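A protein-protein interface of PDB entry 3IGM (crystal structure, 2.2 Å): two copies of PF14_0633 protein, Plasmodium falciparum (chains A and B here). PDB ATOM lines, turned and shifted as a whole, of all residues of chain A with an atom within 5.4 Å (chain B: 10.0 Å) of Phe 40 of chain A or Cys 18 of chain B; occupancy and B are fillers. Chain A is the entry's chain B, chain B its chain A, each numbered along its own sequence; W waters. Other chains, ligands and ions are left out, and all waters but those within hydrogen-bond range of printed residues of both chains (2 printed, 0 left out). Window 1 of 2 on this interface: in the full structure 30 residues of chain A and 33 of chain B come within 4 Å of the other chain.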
ATOM      1  N   CYS A  18     -34.608 -12.453  18.279  1.00  0.00           N
ATOM      2  CA  CYS A  18     -33.745 -12.524  19.452  1.00  0.00           C
ATOM      3  C   CYS A  18     -33.301 -11.095  19.840  1.00  0.00           C
ATOM      4  O   CYS A  18     -32.111 -10.811  20.008  1.00  0.00           O
ATOM      5  CB  CYS A  18     -32.555 -13.447  19.165  1.00  0.00           C
ATOM      6  SG  CYS A  18     -31.555 -13.847  20.601  1.00  0.00           S
ATOM      7  N   HIS A  36     -30.701  -5.557  19.784  1.00  0.00           N
ATOM      8  CA  HIS A  36     -30.096  -6.885  19.918  1.00  0.00           C
ATOM      9  C   HIS A  36     -29.151  -6.911  21.115  1.00  0.00           C
ATOM     10  O   HIS A  36     -28.493  -5.899  21.407  1.00  0.00           O
ATOM     11  CB  HIS A  36     -29.289  -7.242  18.664  1.00  0.00           C
ATOM     12  CG  HIS A  36     -30.137  -7.548  17.471  1.00  0.00           C
ATOM     13  ND1 HIS A  36     -30.729  -8.777  17.275  1.00  0.00           N
ATOM     14  CD2 HIS A  36     -30.504  -6.780  16.418  1.00  0.00           C
ATOM     15  CE1 HIS A  36     -31.416  -8.758  16.148  1.00  0.00           C
ATOM     16  NE2 HIS A  36     -31.292  -7.559  15.606  1.00  0.00           N
ATOM     17  N   PRO A  37     -29.058  -8.069  21.801  1.00  0.00           N
ATOM     18  CA  PRO A  37     -28.010  -8.188  22.804  1.00  0.00           C
ATOM     19  C   PRO A  37     -26.682  -7.724  22.225  1.00  0.00           C
ATOM     20  O   PRO A  37     -26.356  -8.008  21.056  1.00  0.00           O
ATOM     21  CB  PRO A  37     -27.976  -9.686  23.105  1.00  0.00           C
ATOM     22  CG  PRO A  37     -29.372 -10.153  22.835  1.00  0.00           C
ATOM     23  CD  PRO A  37     -29.887  -9.287  21.710  1.00  0.00           C
ATOM     24  N   LYS A  38     -25.941  -6.981  23.031  1.00  0.00           N
ATOM     25  CA  LYS A  38     -24.634  -6.480  22.650  1.00  0.00           C
ATOM     26  C   LYS A  38     -23.749  -7.645  22.217  1.00  0.00           C
ATOM     27  O   LYS A  38     -23.744  -8.701  22.866  1.00  0.00           O
ATOM     28  CB  LYS A  38     -24.005  -5.722  23.826  1.00  0.00           C
ATOM     29  CG  LYS A  38     -24.980  -4.800  24.584  1.00  0.00           C
ATOM     30  CD  LYS A  38     -25.548  -3.691  23.691  1.00  0.00           C
ATOM     31  CE  LYS A  38     -26.532  -2.807  24.459  1.00  0.00           C
ATOM     32  NZ  LYS A  38     -27.268  -1.876  23.543  1.00  0.00           N
ATOM     33  N   HIS A  39     -23.038  -7.450  21.104  1.00  0.00           N
ATOM     34  CA  HIS A  39     -22.115  -8.442  20.539  1.00  0.00           C
ATOM     35  C   HIS A  39     -22.772  -9.800  20.253  1.00  0.00           C
ATOM     36  O   HIS A  39     -22.107 -10.840  20.348  1.00  0.00           O
ATOM     37  CB  HIS A  39     -20.880  -8.650  21.442  1.00  0.00           C
ATOM     38  CG  HIS A  39     -20.271  -7.380  21.956  1.00  0.00           C
ATOM     39  ND1 HIS A  39     -19.480  -6.564  21.178  1.00  0.00           N
ATOM     40  CD2 HIS A  39     -20.328  -6.794  23.177  1.00  0.00           C
ATOM     41  CE1 HIS A  39     -19.078  -5.529  21.895  1.00  0.00           C
ATOM     42  NE2 HIS A  39     -19.581  -5.644  23.112  1.00  0.00           N
ATOM     43  N   PHE A  40     -24.061  -9.798  19.903  1.00  0.00           N
ATOM     44  CA  PHE A  40     -24.762 -11.063  19.675  1.00  0.00           C
ATOM     45  C   PHE A  40     -24.123 -11.885  18.555  1.00  0.00           C
ATOM     46  O   PHE A  40     -23.894 -13.076  18.731  1.00  0.00           O
ATOM     47  CB  PHE A  40     -26.265 -10.886  19.423  1.00  0.00           C
ATOM     48  CG  PHE A  40     -26.995 -12.198  19.246  1.00  0.00           C
ATOM     49  CD1 PHE A  40     -27.208 -13.045  20.337  1.00  0.00           C
ATOM     50  CD2 PHE A  40     -27.432 -12.609  17.987  1.00  0.00           C
ATOM     51  CE1 PHE A  40     -27.863 -14.264  20.184  1.00  0.00           C
ATOM     52  CE2 PHE A  40     -28.096 -13.832  17.824  1.00  0.00           C
ATOM     53  CZ  PHE A  40     -28.304 -14.662  18.923  1.00  0.00           C
ATOM     54  N   ASN A  41     -23.826 -11.240  17.428  1.00  0.00           N
ATOM     55  CA  ASN A  41     -23.198 -11.912  16.291  1.00  0.00           C
ATOM     56  C   ASN A  41     -21.867 -12.568  16.662  1.00  0.00           C
ATOM     57  O   ASN A  41     -21.698 -13.769  16.448  1.00  0.00           O
ATOM     58  CB  ASN A  41     -23.019 -10.941  15.123  1.00  0.00           C
ATOM     59  CG  ASN A  41     -24.331 -10.321  14.674  1.00  0.00           C
ATOM     60  OD1 ASN A  41     -25.389 -10.963  14.704  1.00  0.00           O
ATOM     61  ND2 ASN A  41     -24.270  -9.061  14.258  1.00  0.00           N
ATOM     62  N   MET A  42     -20.947 -11.781  17.235  1.00  0.00           N
ATOM     63  CA  MET A  42     -19.655 -12.288  17.729  1.00  0.00           C
ATOM     64  C   MET A  42     -19.838 -13.522  18.611  1.00  0.00           C
ATOM     65  O   MET A  42     -19.260 -14.582  18.345  1.00  0.00           O
ATOM     66  CB  MET A  42     -18.918 -11.231  18.560  1.00  0.00           C
ATOM     67  CG  MET A  42     -18.348 -10.039  17.812  1.00  0.00           C
ATOM     68  SD  MET A  42     -16.862  -9.377  18.627  1.00  0.00           S
ATOM     69  CE  MET A  42     -17.410  -9.120  20.320  1.00  0.00           C
ATOM     70  N   ASP A  43     -20.645 -13.372  19.659  1.00  0.00           N
ATOM     71  CA  ASP A  43     -20.801 -14.416  20.674  1.00  0.00           C
ATOM     72  C   ASP A  43     -21.564 -15.650  20.183  1.00  0.00           C
ATOM     73  O   ASP A  43     -21.302 -16.762  20.651  1.00  0.00           O
ATOM     74  CB  ASP A  43     -21.412 -13.845  21.962  1.00  0.00           C
ATOM     75  CG  ASP A  43     -20.439 -12.931  22.725  1.00  0.00           C
ATOM     76  OD1 ASP A  43     -19.219 -12.921  22.409  1.00  0.00           O
ATOM     77  OD2 ASP A  43     -20.898 -12.219  23.650  1.00  0.00           O
ATOM     78  N   LYS A  44     -22.490 -15.454  19.242  1.00  0.00           N
ATOM     79  CA  LYS A  44     -23.202 -16.571  18.615  1.00  0.00           C
ATOM     80  C   LYS A  44     -22.234 -17.384  17.751  1.00  0.00           C
ATOM     81  O   LYS A  44     -22.219 -18.618  17.810  1.00  0.00           O
ATOM     82  CB  LYS A  44     -24.398 -16.084  17.780  1.00  0.00           C
ATOM     83  CG  LYS A  44     -25.270 -17.215  17.195  1.00  0.00           C
ATOM     84  CD  LYS A  44     -26.445 -16.649  16.397  1.00  0.00           C
ATOM     85  CE  LYS A  44     -27.240 -17.752  15.703  1.00  0.00           C
ATOM     86  NZ  LYS A  44     -28.121 -17.208  14.632  1.00  0.00           N
ATOM     87  N   GLU A  45     -21.426 -16.675  16.966  1.00  0.00           N
ATOM     88  CA  GLU A  45     -20.401 -17.295  16.136  1.00  0.00           C
ATOM     89  C   GLU A  45     -19.343 -18.050  16.950  1.00  0.00           C
ATOM     90  O   GLU A  45     -18.937 -19.154  16.563  1.00  0.00           O
ATOM     91  CB  GLU A  45     -19.755 -16.258  15.205  1.00  0.00           C
ATOM     92  CG  GLU A  45     -18.682 -16.816  14.250  1.00  0.00           C
ATOM     93  CD  GLU A  45     -19.097 -18.127  13.574  1.00  0.00           C
ATOM     94  OE1 GLU A  45     -20.272 -18.261  13.151  1.00  0.00           O
ATOM     95  OE2 GLU A  45     -18.239 -19.029  13.472  1.00  0.00           O
ATOM     96  N   SER B  12     -26.929 -27.889  15.509  1.00  0.00           N
ATOM     97  CA  SER B  12     -28.065 -27.085  15.084  1.00  0.00           C
ATOM     98  C   SER B  12     -28.479 -26.047  16.114  1.00  0.00           C
ATOM     99  O   SER B  12     -28.344 -26.256  17.323  1.00  0.00           O
ATOM    100  CB  SER B  12     -29.261 -27.967  14.675  1.00  0.00           C
ATOM    101  OG  SER B  12     -29.685 -28.818  15.720  1.00  0.00           O
ATOM    102  N   TRP B  13     -28.976 -24.922  15.601  1.00  0.00           N
ATOM    103  CA  TRP B  13     -29.556 -23.847  16.399  1.00  0.00           C
ATOM    104  C   TRP B  13     -30.952 -24.211  16.922  1.00  0.00           C
ATOM    105  O   TRP B  13     -31.854 -24.507  16.141  1.00  0.00           O
ATOM    106  CB  TRP B  13     -29.656 -22.598  15.527  1.00  0.00           C
ATOM    107  CG  TRP B  13     -30.038 -21.352  16.247  1.00  0.00           C
ATOM    108  CD1 TRP B  13     -31.187 -20.630  16.086  1.00  0.00           C
ATOM    109  CD2 TRP B  13     -29.262 -20.660  17.227  1.00  0.00           C
ATOM    110  NE1 TRP B  13     -31.179 -19.533  16.913  1.00  0.00           N
ATOM    111  CE2 TRP B  13     -30.007 -19.525  17.624  1.00  0.00           C
ATOM    112  CE3 TRP B  13     -28.008 -20.887  17.812  1.00  0.00           C
ATOM    113  CZ2 TRP B  13     -29.534 -18.614  18.572  1.00  0.00           C
ATOM    114  CZ3 TRP B  13     -27.539 -19.980  18.762  1.00  0.00           C
ATOM    115  CH2 TRP B  13     -28.302 -18.858  19.129  1.00  0.00           C
ATOM    116  N   ASN B  14     -31.107 -24.200  18.247  1.00  0.00           N
ATOM    117  CA  ASN B  14     -32.406 -24.339  18.898  1.00  0.00           C
ATOM    118  C   ASN B  14     -32.930 -22.933  19.209  1.00  0.00           C
ATOM    119  O   ASN B  14     -32.363 -22.223  20.040  1.00  0.00           O
ATOM    120  CB  ASN B  14     -32.279 -25.203  20.163  1.00  0.00           C
ATOM    121  CG  ASN B  14     -33.619 -25.459  20.851  1.00  0.00           C
ATOM    122  OD1 ASN B  14     -34.328 -24.526  21.217  1.00  0.00           O
ATOM    123  ND2 ASN B  14     -33.954 -26.734  21.048  1.00  0.00           N
ATOM    124  N   LYS B  15     -33.992 -22.537  18.506  1.00  0.00           N
ATOM    125  CA  LYS B  15     -34.529 -21.168  18.548  1.00  0.00           C
ATOM    126  C   LYS B  15     -35.056 -20.744  19.925  1.00  0.00           C
ATOM    127  O   LYS B  15     -34.691 -19.677  20.424  1.00  0.00           O
ATOM    128  CB  LYS B  15     -35.631 -20.991  17.500  1.00  0.00           C
ATOM    129  CG  LYS B  15     -35.140 -20.652  16.102  1.00  0.00           C
ATOM    130  CD  LYS B  15     -36.316 -20.617  15.125  1.00  0.00           C
ATOM    131  CE  LYS B  15     -35.839 -20.474  13.684  1.00  0.00           C
ATOM    132  NZ  LYS B  15     -36.921 -20.819  12.712  1.00  0.00           N
ATOM    133  N   ARG B  16     -35.909 -21.578  20.523  1.00  0.00           N
ATOM    134  CA  ARG B  16     -36.447 -21.320  21.866  1.00  0.00           C
ATOM    135  C   ARG B  16     -35.312 -21.166  22.890  1.00  0.00           C
ATOM    136  O   ARG B  16     -35.332 -20.256  23.716  1.00  0.00           O
ATOM    137  CB  ARG B  16     -37.405 -22.439  22.296  1.00  0.00           C
ATOM    138  CG  ARG B  16     -38.185 -22.164  23.588  1.00  0.00           C
ATOM    139  CD  ARG B  16     -38.625 -23.476  24.243  1.00  0.00           C
ATOM    140  NE  ARG B  16     -37.523 -24.125  24.954  1.00  0.00           N
ATOM    141  CZ  ARG B  16     -37.536 -25.378  25.412  1.00  0.00           C
ATOM    142  NH1 ARG B  16     -38.600 -26.156  25.234  1.00  0.00           N
ATOM    143  NH2 ARG B  16     -36.468 -25.860  26.047  1.00  0.00           N
ATOM    144  N   MET B  17     -34.320 -22.051  22.815  1.00  0.00           N
ATOM    145  CA  MET B  17     -33.173 -22.010  23.714  1.00  0.00           C
ATOM    146  C   MET B  17     -32.211 -20.864  23.418  1.00  0.00           C
ATOM    147  O   MET B  17     -31.486 -20.428  24.311  1.00  0.00           O
ATOM    148  CB  MET B  17     -32.413 -23.330  23.665  1.00  0.00           C
ATOM    149  CG  MET B  17     -33.159 -24.479  24.275  1.00  0.00           C
ATOM    150  SD  MET B  17     -32.131 -25.946  24.351  1.00  0.00           S
ATOM    151  CE  MET B  17     -31.076 -25.499  25.734  1.00  0.00           C
ATOM    152  N   CYS B  18     -32.222 -20.378  22.174  1.00  0.00           N
ATOM    153  CA  CYS B  18     -31.215 -19.435  21.670  1.00  0.00           C
ATOM    154  C   CYS B  18     -29.784 -19.988  21.886  1.00  0.00           C
ATOM    155  O   CYS B  18     -28.894 -19.301  22.419  1.00  0.00           O
ATOM    156  CB  CYS B  18     -31.407 -18.033  22.280  1.00  0.00           C
ATOM    157  SG  CYS B  18     -30.740 -16.658  21.257  1.00  0.00           S
ATOM    158  N   ALA B  19     -29.575 -21.233  21.459  1.00  0.00           N
ATOM    159  CA  ALA B  19     -28.327 -21.956  21.719  1.00  0.00           C
ATOM    160  C   ALA B  19     -28.040 -23.033  20.679  1.00  0.00           C
ATOM    161  O   ALA B  19     -28.960 -23.641  20.119  1.00  0.00           O
ATOM    162  CB  ALA B  19     -28.346 -22.577  23.115  1.00  0.00           C
ATOM    163  N   TRP B  20     -26.754 -23.266  20.436  1.00  0.00           N
ATOM    164  CA  TRP B  20     -26.319 -24.350  19.572  1.00  0.00           C
ATOM    165  C   TRP B  20     -26.377 -25.657  20.340  1.00  0.00           C
ATOM    166  O   TRP B  20     -25.913 -25.741  21.484  1.00  0.00           O
ATOM    167  CB  TRP B  20     -24.888 -24.119  19.083  1.00  0.00           C
ATOM    168  CG  TRP B  20     -24.707 -22.873  18.258  1.00  0.00           C
ATOM    169  CD1 TRP B  20     -24.103 -21.717  18.652  1.00  0.00           C
ATOM    170  CD2 TRP B  20     -25.127 -22.665  16.903  1.00  0.00           C
ATOM    171  NE1 TRP B  20     -24.109 -20.802  17.628  1.00  0.00           N
ATOM    172  CE2 TRP B  20     -24.735 -21.353  16.542  1.00  0.00           C
ATOM    173  CE3 TRP B  20     -25.793 -23.455  15.957  1.00  0.00           C
ATOM    174  CZ2 TRP B  20     -24.987 -20.813  15.272  1.00  0.00           C
ATOM    175  CZ3 TRP B  20     -26.048 -22.912  14.692  1.00  0.00           C
ATOM    176  CH2 TRP B  20     -25.641 -21.607  14.366  1.00  0.00           C
ATOM    177  N   LEU B  21     -26.960 -26.672  19.710  1.00  0.00           N
ATOM    178  CA  LEU B  21     -26.949 -28.018  20.265  1.00  0.00           C
ATOM    179  C   LEU B  21     -26.106 -28.944  19.395  1.00  0.00           C
ATOM    180  O   LEU B  21     -26.260 -28.975  18.171  1.00  0.00           O
ATOM    181  CB  LEU B  21     -28.376 -28.570  20.400  1.00  0.00           C
ATOM    182  CG  LEU B  21     -29.270 -28.244  21.608  1.00  0.00           C
ATOM    183  CD1 LEU B  21     -28.828 -29.045  22.813  1.00  0.00           C
ATOM    184  CD2 LEU B  21     -29.352 -26.745  21.929  1.00  0.00           C
ATOM    185  N   THR B  34     -25.418 -28.562  24.987  1.00  0.00           N
ATOM    186  CA  THR B  34     -25.906 -27.217  24.707  1.00  0.00           C
ATOM    187  C   THR B  34     -24.802 -26.152  24.782  1.00  0.00           C
ATOM    188  O   THR B  34     -23.978 -26.154  25.707  1.00  0.00           O
ATOM    189  CB  THR B  34     -27.049 -26.859  25.689  1.00  0.00           C
ATOM    190  OG1 THR B  34     -28.124 -27.796  25.535  1.00  0.00           O
ATOM    191  CG2 THR B  34     -27.562 -25.437  25.456  1.00  0.00           C
ATOM    192  N   PHE B  35     -24.818 -25.234  23.814  1.00  0.00           N
ATOM    193  CA  PHE B  35     -23.840 -24.153  23.728  1.00  0.00           C
ATOM    194  C   PHE B  35     -24.505 -22.791  23.516  1.00  0.00           C
ATOM    195  O   PHE B  35     -24.774 -22.399  22.381  1.00  0.00           O
ATOM    196  CB  PHE B  35     -22.827 -24.431  22.603  1.00  0.00           C
ATOM    197  CG  PHE B  35     -21.919 -25.603  22.871  1.00  0.00           C
ATOM    198  CD1 PHE B  35     -20.694 -25.421  23.521  1.00  0.00           C
ATOM    199  CD2 PHE B  35     -22.278 -26.891  22.464  1.00  0.00           C
ATOM    200  CE1 PHE B  35     -19.845 -26.499  23.765  1.00  0.00           C
ATOM    201  CE2 PHE B  35     -21.427 -27.982  22.708  1.00  0.00           C
ATOM    202  CZ  PHE B  35     -20.214 -27.781  23.364  1.00  0.00           C
ATOM    203  N   HIS B  36     -24.763 -22.079  24.619  1.00  0.00           N
ATOM    204  CA  HIS B  36     -25.294 -20.703  24.578  1.00  0.00           C
ATOM    205  C   HIS B  36     -24.191 -19.737  24.177  1.00  0.00           C
ATOM    206  O   HIS B  36     -23.021 -19.982  24.499  1.00  0.00           O
ATOM    207  CB  HIS B  36     -25.832 -20.271  25.956  1.00  0.00           C
ATOM    208  CG  HIS B  36     -27.126 -20.920  26.335  1.00  0.00           C
ATOM    209  ND1 HIS B  36     -28.354 -20.375  26.021  1.00  0.00           N
ATOM    210  CD2 HIS B  36     -27.385 -22.072  26.997  1.00  0.00           C
ATOM    211  CE1 HIS B  36     -29.310 -21.164  26.474  1.00  0.00           C
ATOM    212  NE2 HIS B  36     -28.749 -22.204  27.065  1.00  0.00           N
ATOM    213  N   PRO B  37     -24.550 -18.631  23.484  1.00  0.00           N
ATOM    214  CA  PRO B  37     -23.561 -17.560  23.327  1.00  0.00           C
ATOM    215  C   PRO B  37     -23.013 -17.184  24.711  1.00  0.00           C
ATOM    216  O   PRO B  37     -23.783 -17.114  25.671  1.00  0.00           O
ATOM    217  CB  PRO B  37     -24.374 -16.412  22.712  1.00  0.00           C
ATOM    218  CG  PRO B  37     -25.536 -17.090  22.037  1.00  0.00           C
ATOM    219  CD  PRO B  37     -25.855 -18.270  22.897  1.00  0.00           C
ATOM    220  N   LYS B  38     -21.698 -16.978  24.801  1.00  0.00           N
ATOM    221  CA  LYS B  38     -20.974 -16.894  26.086  1.00  0.00           C
ATOM    222  C   LYS B  38     -21.588 -16.012  27.181  1.00  0.00           C
ATOM    223  O   LYS B  38     -21.757 -16.464  28.316  1.00  0.00           O
ATOM    224  CB  LYS B  38     -19.502 -16.516  25.867  1.00  0.00           C
ATOM    225  CG  LYS B  38     -18.599 -17.712  25.566  1.00  0.00           C
ATOM    226  CD  LYS B  38     -17.185 -17.277  25.174  1.00  0.00           C
ATOM    227  CE  LYS B  38     -16.313 -18.487  24.805  1.00  0.00           C
ATOM    228  NZ  LYS B  38     -14.878 -18.118  24.567  1.00  0.00           N
ATOM    229  N   HIS B  39     -21.910 -14.764  26.863  1.00  0.00           N
ATOM    230  CA  HIS B  39     -22.455 -13.882  27.893  1.00  0.00           C
ATOM    231  C   HIS B  39     -23.865 -13.437  27.544  1.00  0.00           C
ATOM    232  O   HIS B  39     -24.215 -12.265  27.707  1.00  0.00           O
ATOM    233  CB  HIS B  39     -21.519 -12.698  28.160  1.00  0.00           C
ATOM    234  CG  HIS B  39     -20.318 -13.055  28.986  1.00  0.00           C
ATOM    235  ND1 HIS B  39     -19.115 -13.436  28.430  1.00  0.00           N
ATOM    236  CD2 HIS B  39     -20.138 -13.095  30.330  1.00  0.00           C
ATOM    237  CE1 HIS B  39     -18.247 -13.696  29.393  1.00  0.00           C
ATOM    238  NE2 HIS B  39     -18.843 -13.497  30.555  1.00  0.00           N
ATOM    239  N   PHE B  40     -24.671 -14.392  27.078  1.00  0.00           N
ATOM    240  CA  PHE B  40     -26.000 -14.096  26.548  1.00  0.00           C
ATOM    241  C   PHE B  40     -26.903 -13.398  27.556  1.00  0.00           C
ATOM    242  O   PHE B  40     -27.516 -12.387  27.235  1.00  0.00           O
ATOM    243  CB  PHE B  40     -26.695 -15.354  26.010  1.00  0.00           C
ATOM    244  CG  PHE B  40     -28.100 -15.101  25.531  1.00  0.00           C
ATOM    245  CD1 PHE B  40     -28.329 -14.542  24.274  1.00  0.00           C
ATOM    246  CD2 PHE B  40     -29.192 -15.387  26.352  1.00  0.00           C
ATOM    247  CE1 PHE B  40     -29.627 -14.288  23.831  1.00  0.00           C
ATOM    248  CE2 PHE B  40     -30.499 -15.140  25.923  1.00  0.00           C
ATOM    249  CZ  PHE B  40     -30.721 -14.588  24.658  1.00  0.00           C
ATOM    250  N   ASN B  41     -26.993 -13.956  28.759  1.00  0.00           N
ATOM    251  CA  ASN B  41     -27.873 -13.410  29.791  1.00  0.00           C
ATOM    252  C   ASN B  41     -27.546 -11.971  30.170  1.00  0.00           C
ATOM    253  O   ASN B  41     -28.448 -11.135  30.280  1.00  0.00           O
ATOM    254  CB  ASN B  41     -27.906 -14.315  31.024  1.00  0.00           C
ATOM    255  CG  ASN B  41     -28.756 -15.565  30.809  1.00  0.00           C
ATOM    256  OD1 ASN B  41     -29.468 -15.694  29.804  1.00  0.00           O
ATOM    257  ND2 ASN B  41     -28.684 -16.493  31.758  1.00  0.00           N
ATOM    258  N   MET B  42     -26.256 -11.700  30.365  1.00  0.00           N
ATOM    259  CA  MET B  42     -25.787 -10.360  30.696  1.00  0.00           C
ATOM    260  C   MET B  42     -26.022  -9.373  29.551  1.00  0.00           C
ATOM    261  O   MET B  42     -26.458  -8.254  29.786  1.00  0.00           O
ATOM    262  CB  MET B  42     -24.303 -10.377  31.086  1.00  0.00           C
ATOM    263  CG  MET B  42     -23.976 -11.257  32.288  1.00  0.00           C
ATOM    264  SD  MET B  42     -22.318 -10.957  32.957  1.00  0.00           S
ATOM    265  CE  MET B  42     -22.611  -9.455  33.911  1.00  0.00           C
ATOM    266  N   ASP B  43     -25.756  -9.798  28.318  1.00  0.00           N
ATOM    267  CA  ASP B  43     -25.841  -8.909  27.156  1.00  0.00           C
ATOM    268  C   ASP B  43     -27.267  -8.664  26.704  1.00  0.00           C
ATOM    269  O   ASP B  43     -27.559  -7.633  26.096  1.00  0.00           O
ATOM    270  CB  ASP B  43     -24.986  -9.435  26.000  1.00  0.00           C
ATOM    271  CG  ASP B  43     -23.488  -9.225  26.236  1.00  0.00           C
ATOM    272  OD1 ASP B  43     -23.108  -8.464  27.168  1.00  0.00           O
ATOM    273  OD2 ASP B  43     -22.692  -9.823  25.476  1.00  0.00           O
ATOM    274  N   LYS B  44     -28.145  -9.622  26.997  1.00  0.00           N
ATOM    275  CA  LYS B  44     -29.569  -9.467  26.741  1.00  0.00           C
ATOM    276  C   LYS B  44     -30.133  -8.434  27.727  1.00  0.00           C
ATOM    277  O   LYS B  44     -30.966  -7.599  27.361  1.00  0.00           O
ATOM    278  CB  LYS B  44     -30.282 -10.818  26.879  1.00  0.00           C
ATOM    279  CG  LYS B  44     -31.783 -10.760  26.753  1.00  0.00           C
ATOM    280  CD  LYS B  44     -32.392 -12.145  26.928  1.00  0.00           C
ATOM    281  CE  LYS B  44     -33.909 -12.072  26.846  1.00  0.00           C
ATOM    282  NZ  LYS B  44     -34.549 -13.417  26.966  1.00  0.00           N
ATOM    283  N   ALA B  47     -29.103  -4.983  26.724  1.00  0.00           N
ATOM    284  CA  ALA B  47     -29.936  -4.568  25.604  1.00  0.00           C
ATOM    285  C   ALA B  47     -31.327  -4.157  26.078  1.00  0.00           C
ATOM    286  O   ALA B  47     -31.894  -3.188  25.568  1.00  0.00           O
ATOM    287  CB  ALA B  47     -30.022  -5.676  24.556  1.00  0.00           C
HETATM  288  O   HOH W   1     -23.521 -13.030  24.571  1.00  0.00           O
HETATM  289  O   HOH W   2     -19.097 -12.781  25.793  1.00  0.00           O
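The backbone carbonyl oxygen of Lys 44 of chain A is in hydrogen-bond range of the indole nitrogen of Trp 20 of chain B.
The side-chain sulfur (SG) of Cys 18 of chain A lies close to the side-chain sulfur (SG) of Cys 18 of chain B (3.0 Å).
The backbone carbonyl oxygen (O) of Lys 38 of chain A sits close to the side-chain carboxylate (OD2) of Asp 43 of chain B, at 3.0 Å.
The backbone NH of Phe 35 of chain B lies within hydrogen-bond range of the backbone carbonyl oxygen of Trp 20 of chain B.
Among the printed residues, merely in contact across the chains: Cys 18 of chain A with Phe 40 of chain B, His 36 of chain A with Ala 47 of chain B, Pro 37 of chain A with Asp 43 of chain B, Pro 37 of chain A with Lys 44 of chain B, Pro 37 of chain A with Ala 47 of chain B, Lys 38 of chain A with Ala 47 of chain B, Phe 40 of chain A with Cys 18 of chain B, Asp 43 of chain A with Pro 37 of chain B, Asp 43 of chain A with Asp 43 of chain B and Lys 44 of chain A with Trp 13 of chain B.
Of chain B, only Cys 18 comes within 4 Å of Phe 40 of chain A.
Cys 18 of chain B touches just these residues of chain A: Cys 18 and Phe 40.
Of chain B, only Asp 43 (3.4 Å), Lys 44 (3.9 Å) and Ala 47 (3.7 Å) come within 4 Å of Pro 37 of chain A.
Asn 41 of chain A touches none of the printed residues of chain B.
Of chain B, only Trp 13 (3.8 Å) and Trp 20 (2.9 Å) come within 4 Å of Lys 44 of chain A.
Of the printed residues of chain A, Trp 20 of chain B touches Lys 44.
Of the printed residues of chain A, Asp 43 of chain B touches Pro 37, Lys 38 and Asp 43.
Of the printed residues of chain A, Phe 40 of chain B touches Cys 18 (3.8 Å).
Of the printed residues of chain A, Lys 44 of chain B touches Pro 37.
Of the printed residues of chain B, Lys 38 of chain A touches Asp 43 and Ala 47.
Lys 38 of chain B touches none of the printed residues of chain A.
The nearest residue of chain B that does not touch Phe 40 of chain A is Phe 40 of chain B (4.1 Å).
Printed residues of chain A that touch a printed residue of chain B: Cys 18, His 36, Pro 37, Lys 38, Phe 40, Asp 43 and Lys 44.
Hydrophobic or aromatic side chains of chain B within 4 Å of the printed part of chain A: Trp 13, Trp 20, Pro 37, Phe 40 and Ala 47.
Pro 37 of chain A touches Asp 43 of chain B, and with the chains exchanged Asp 43 of chain A touches Pro 37 of chain B.
Pro 37 of chain A touches Lys 44 of chain B, but with the chains exchanged Lys 44 of chain A does not touch Pro 37 of chain B (4.1 Å).
Lys 38 of chain A touches Asp 43 of chain B, but with the chains exchanged Asp 43 of chain A does not touch Lys 38 of chain B (4.2 Å).
Asp 43 of chain A touches its own counterpart, Asp 43 of chain B.
10 positions are printed for both chains.
Water W2 bridges ND1 of His 39 of chain B (2.7 Å) and OD2 of Asp 43 of chain A (2.9 Å).
Water W1 lies within hydrogen-bond range of OD2 of Asp 43 of chain A, N of Phe 40 of chain B, N of His 39 of chain B and OD2 of Asp 43 of chain B.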
